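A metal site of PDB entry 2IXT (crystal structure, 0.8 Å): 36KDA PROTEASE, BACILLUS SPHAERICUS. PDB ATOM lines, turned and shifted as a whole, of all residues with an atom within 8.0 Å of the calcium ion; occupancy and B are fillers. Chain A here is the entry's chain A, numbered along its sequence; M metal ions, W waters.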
ATOM      1  N   TYR A 211     -22.145 -27.494 -10.103  1.00  0.00           N
ATOM      2  CA  TYR A 211     -21.918 -28.187 -11.373  1.00  0.00           C
ATOM      3  C   TYR A 211     -21.393 -27.231 -12.429  1.00  0.00           C
ATOM      4  O   TYR A 211     -21.831 -26.091 -12.569  1.00  0.00           O
ATOM      5  CB  TYR A 211     -23.256 -28.795 -11.865  1.00  0.00           C
ATOM      6  CG  TYR A 211     -23.774 -29.876 -10.937  1.00  0.00           C
ATOM      7  CD1 TYR A 211     -24.601 -29.546  -9.841  1.00  0.00           C
ATOM      8  CD2 TYR A 211     -23.416 -31.205 -11.110  1.00  0.00           C
ATOM      9  CE1 TYR A 211     -25.076 -30.544  -9.004  1.00  0.00           C
ATOM     10  CE2 TYR A 211     -23.899 -32.193 -10.270  1.00  0.00           C
ATOM     11  CZ  TYR A 211     -24.735 -31.858  -9.227  1.00  0.00           C
ATOM     12  OH  TYR A 211     -25.180 -32.857  -8.397  1.00  0.00           O
ATOM     13  N   ILE A 212     -20.455 -27.717 -13.246  1.00  0.00           N
ATOM     14  CA  ILE A 212     -19.914 -26.923 -14.322  1.00  0.00           C
ATOM     15  C   ILE A 212     -20.982 -26.433 -15.297  1.00  0.00           C
ATOM     16  O   ILE A 212     -20.951 -25.259 -15.723  1.00  0.00           O
ATOM     17  CB  ILE A 212     -18.815 -27.715 -15.051  1.00  0.00           C
ATOM     18  CG1 ILE A 212     -17.581 -27.737 -14.174  1.00  0.00           C
ATOM     19  CG2 ILE A 212     -18.512 -27.138 -16.441  1.00  0.00           C
ATOM     20  CD1 ILE A 212     -16.515 -28.751 -14.595  1.00  0.00           C
ATOM     21  N   SER A 213     -21.877 -27.314 -15.703  1.00  0.00           N
ATOM     22  CA  SER A 213     -22.721 -26.981 -16.853  1.00  0.00           C
ATOM     23  C   SER A 213     -23.543 -25.733 -16.649  1.00  0.00           C
ATOM     24  O   SER A 213     -23.723 -24.973 -17.605  1.00  0.00           O
ATOM     25  CB  SER A 213     -23.636 -28.151 -17.161  1.00  0.00           C
ATOM     26  OG  SER A 213     -24.505 -28.438 -16.059  1.00  0.00           O
ATOM     27  N   THR A 214     -24.063 -25.536 -15.428  1.00  0.00           N
ATOM     28  CA  THR A 214     -24.961 -24.431 -15.172  1.00  0.00           C
ATOM     29  C   THR A 214     -24.290 -23.263 -14.460  1.00  0.00           C
ATOM     30  O   THR A 214     -24.964 -22.271 -14.224  1.00  0.00           O
ATOM     31  CB  THR A 214     -26.187 -24.922 -14.395  1.00  0.00           C
ATOM     32  OG1 THR A 214     -25.735 -25.557 -13.212  1.00  0.00           O
ATOM     33  CG2 THR A 214     -27.025 -25.885 -15.196  1.00  0.00           C
ATOM     34  N   ALA A 215     -23.018 -23.374 -14.114  1.00  0.00           N
ATOM     35  CA  ALA A 215     -22.319 -22.220 -13.547  1.00  0.00           C
ATOM     36  C   ALA A 215     -21.928 -21.253 -14.670  1.00  0.00           C
ATOM     37  O   ALA A 215     -21.627 -21.701 -15.773  1.00  0.00           O
ATOM     38  CB  ALA A 215     -21.106 -22.666 -12.761  1.00  0.00           C
ATOM     39  N   GLY A 216     -21.868 -19.975 -14.342  1.00  0.00           N
ATOM     40  CA  GLY A 216     -21.267 -18.962 -15.170  1.00  0.00           C
ATOM     41  C   GLY A 216     -22.165 -17.897 -15.691  1.00  0.00           C
ATOM     42  O   GLY A 216     -21.696 -16.837 -16.100  1.00  0.00           O
ATOM     43  N   ASP A 217     -23.471 -18.142 -15.658  1.00  0.00           N
ATOM     44  CA  ASP A 217     -24.457 -17.278 -16.224  1.00  0.00           C
ATOM     45  C   ASP A 217     -25.054 -16.258 -15.258  1.00  0.00           C
ATOM     46  O   ASP A 217     -25.879 -15.435 -15.676  1.00  0.00           O
ATOM     47  CB  ASP A 217     -25.619 -18.081 -16.895  1.00  0.00           C
ATOM     48  CG  ASP A 217     -26.365 -19.003 -15.949  1.00  0.00           C
ATOM     49  OD1 ASP A 217     -27.453 -19.480 -16.368  1.00  0.00           O
ATOM     50  OD2 ASP A 217     -25.860 -19.246 -14.837  1.00  0.00           O
ATOM     51  N   TYR A 218     -24.674 -16.316 -13.983  1.00  0.00           N
ATOM     52  CA  TYR A 218     -25.303 -15.454 -12.983  1.00  0.00           C
ATOM     53  C   TYR A 218     -26.839 -15.573 -12.970  1.00  0.00           C
ATOM     54  O   TYR A 218     -27.525 -14.617 -12.674  1.00  0.00           O
ATOM     55  CB  TYR A 218     -24.868 -13.978 -13.083  1.00  0.00           C
ATOM     56  CG  TYR A 218     -23.419 -13.705 -12.748  1.00  0.00           C
ATOM     57  CD1 TYR A 218     -22.475 -13.557 -13.737  1.00  0.00           C
ATOM     58  CD2 TYR A 218     -23.002 -13.587 -11.450  1.00  0.00           C
ATOM     59  CE1 TYR A 218     -21.158 -13.227 -13.456  1.00  0.00           C
ATOM     60  CE2 TYR A 218     -21.681 -13.276 -11.115  1.00  0.00           C
ATOM     61  CZ  TYR A 218     -20.763 -13.086 -12.141  1.00  0.00           C
ATOM     62  OH  TYR A 218     -19.463 -12.708 -11.870  1.00  0.00           O
ATOM     63  N   VAL A 219     -27.330 -16.802 -13.190  1.00  0.00           N
ATOM     64  CA  VAL A 219     -28.750 -17.107 -13.052  1.00  0.00           C
ATOM     65  C   VAL A 219     -28.808 -18.456 -12.349  1.00  0.00           C
ATOM     66  O   VAL A 219     -28.150 -19.399 -12.759  1.00  0.00           O
ATOM     67  CB  VAL A 219     -29.457 -17.211 -14.411  1.00  0.00           C
ATOM     68  CG1 VAL A 219     -30.936 -17.595 -14.182  1.00  0.00           C
ATOM     69  CG2 VAL A 219     -29.388 -15.861 -15.144  1.00  0.00           C
ATOM     70  N   ILE A 220     -29.583 -18.566 -11.275  1.00  0.00           N
ATOM     71  CA  ILE A 220     -29.586 -19.795 -10.466  1.00  0.00           C
ATOM     72  C   ILE A 220     -30.533 -20.836 -11.014  1.00  0.00           C
ATOM     73  O   ILE A 220     -31.739 -20.653 -11.070  1.00  0.00           O
ATOM     74  CB  ILE A 220     -29.943 -19.476  -8.997  1.00  0.00           C
ATOM     75  CG1 ILE A 220     -28.879 -18.593  -8.343  1.00  0.00           C
ATOM     76  CG2 ILE A 220     -30.143 -20.763  -8.166  1.00  0.00           C
ATOM     77  CD1 ILE A 220     -27.513 -19.225  -8.211  1.00  0.00           C
ATOM     78  N   GLN A 221     -29.942 -21.971 -11.377  1.00  0.00           N
ATOM     79  CA  GLN A 221     -30.652 -23.207 -11.671  1.00  0.00           C
ATOM     80  C   GLN A 221     -30.443 -24.196 -10.522  1.00  0.00           C
ATOM     81  O   GLN A 221     -29.607 -23.979  -9.624  1.00  0.00           O
ATOM     82  CB  GLN A 221     -30.161 -23.834 -12.985  1.00  0.00           C
ATOM     83  CG  GLN A 221     -30.505 -22.976 -14.212  1.00  0.00           C
ATOM     84  CD  GLN A 221     -29.450 -21.945 -14.576  1.00  0.00           C
ATOM     85  OE1 GLN A 221     -28.259 -22.117 -14.273  1.00  0.00           O
ATOM     86  NE2 GLN A 221     -29.839 -20.899 -15.265  1.00  0.00           N
ATOM     87  N   GLU A 222     -31.149 -25.331 -10.580  1.00  0.00           N
ATOM     88  CA  GLU A 222     -30.936 -26.382  -9.625  1.00  0.00           C
ATOM     89  C   GLU A 222     -29.475 -26.804  -9.646  1.00  0.00           C
ATOM     90  O   GLU A 222     -28.907 -27.006 -10.756  1.00  0.00           O
ATOM     91  CB  GLU A 222     -31.850 -27.562  -9.953  1.00  0.00           C
ATOM     92  CG  GLU A 222     -31.710 -28.738  -8.984  1.00  0.00           C
ATOM     93  CD  GLU A 222     -32.765 -29.823  -9.145  1.00  0.00           C
ATOM     94  OE1 GLU A 222     -32.644 -30.851  -8.483  1.00  0.00           O
ATOM     95  OE2 GLU A 222     -33.787 -29.603  -9.836  1.00  0.00           O
ATOM     96  N   GLY A 223     -28.865 -26.955  -8.475  1.00  0.00           N
ATOM     97  CA  GLY A 223     -27.488 -27.363  -8.371  1.00  0.00           C
ATOM     98  C   GLY A 223     -26.455 -26.271  -8.294  1.00  0.00           C
ATOM     99  O   GLY A 223     -25.266 -26.557  -8.115  1.00  0.00           O
ATOM    100  N   ASP A 224     -26.877 -25.007  -8.398  1.00  0.00           N
ATOM    101  CA  ASP A 224     -25.938 -23.893  -8.380  1.00  0.00           C
ATOM    102  C   ASP A 224     -25.724 -23.333  -6.968  1.00  0.00           C
ATOM    103  O   ASP A 224     -26.675 -23.078  -6.205  1.00  0.00           O
ATOM    104  CB  ASP A 224     -26.469 -22.743  -9.210  1.00  0.00           C
ATOM    105  CG  ASP A 224     -26.443 -22.989 -10.708  1.00  0.00           C
ATOM    106  OD1 ASP A 224     -27.085 -22.173 -11.421  1.00  0.00           O
ATOM    107  OD2 ASP A 224     -25.776 -23.954 -11.166  1.00  0.00           O
ATOM    108  N   ILE A 225     -24.444 -23.110  -6.669  1.00  0.00           N
ATOM    109  CA  ILE A 225     -24.044 -22.297  -5.524  1.00  0.00           C
ATOM    110  C   ILE A 225     -24.404 -20.846  -5.818  1.00  0.00           C
ATOM    111  O   ILE A 225     -24.295 -20.404  -6.965  1.00  0.00           O
ATOM    112  CB  ILE A 225     -22.533 -22.452  -5.292  1.00  0.00           C
ATOM    113  CG1 ILE A 225     -22.138 -23.911  -5.070  1.00  0.00           C
ATOM    114  CG2 ILE A 225     -22.040 -21.548  -4.153  1.00  0.00           C
ATOM    115  CD1 ILE A 225     -22.562 -24.496  -3.747  1.00  0.00           C
ATOM    116  N   ASP A 298     -18.986 -16.024 -12.089  1.00  0.00           N
ATOM    117  CA  ASP A 298     -19.849 -16.962 -11.369  1.00  0.00           C
ATOM    118  C   ASP A 298     -19.274 -18.354 -11.534  1.00  0.00           C
ATOM    119  O   ASP A 298     -19.052 -18.775 -12.677  1.00  0.00           O
ATOM    120  CB  ASP A 298     -21.247 -16.839 -12.000  1.00  0.00           C
ATOM    121  CG  ASP A 298     -22.234 -17.877 -11.571  1.00  0.00           C
ATOM    122  OD1 ASP A 298     -23.161 -18.171 -12.394  1.00  0.00           O
ATOM    123  OD2 ASP A 298     -22.103 -18.384 -10.438  1.00  0.00           O
ATOM    124  N   PHE A 304     -21.921 -16.620  -7.096  1.00  0.00           N
ATOM    125  CA  PHE A 304     -21.792 -15.294  -7.647  1.00  0.00           C
ATOM    126  C   PHE A 304     -20.665 -14.519  -7.000  1.00  0.00           C
ATOM    127  O   PHE A 304     -20.147 -13.584  -7.643  1.00  0.00           O
ATOM    128  CB  PHE A 304     -23.117 -14.537  -7.482  1.00  0.00           C
ATOM    129  CG  PHE A 304     -24.269 -15.032  -8.322  1.00  0.00           C
ATOM    130  CD1 PHE A 304     -24.310 -16.276  -8.954  1.00  0.00           C
ATOM    131  CD2 PHE A 304     -25.384 -14.215  -8.443  1.00  0.00           C
ATOM    132  CE1 PHE A 304     -25.439 -16.705  -9.643  1.00  0.00           C
ATOM    133  CE2 PHE A 304     -26.500 -14.609  -9.193  1.00  0.00           C
ATOM    134  CZ  PHE A 304     -26.539 -15.884  -9.745  1.00  0.00           C
HETATM  135 CA    CA M   1     -26.544 -20.912 -13.311  1.00  0.00          CA
HETATM  136  O   HOH W   1     -25.021 -19.944 -11.833  1.00  0.00           O
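The backbone NH (N) of Asp 217 lies within hydrogen-bond range of the side-chain carboxylate (OD1) of Asp 298, at 3.3 Å.
The calcium ion is bound by the backbone carbonyl oxygen of Val 219 (2.3 Å), the backbone carbonyl oxygen of Thr 214 (2.3 Å), the side-chain amide oxygen of Gln 221 (2.3 Å), water W1 (2.3 Å), the side-chain carboxylate of Asp 224 (2.3 Å) and the side-chain carboxylate of Asp 217 (2.4 Å).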
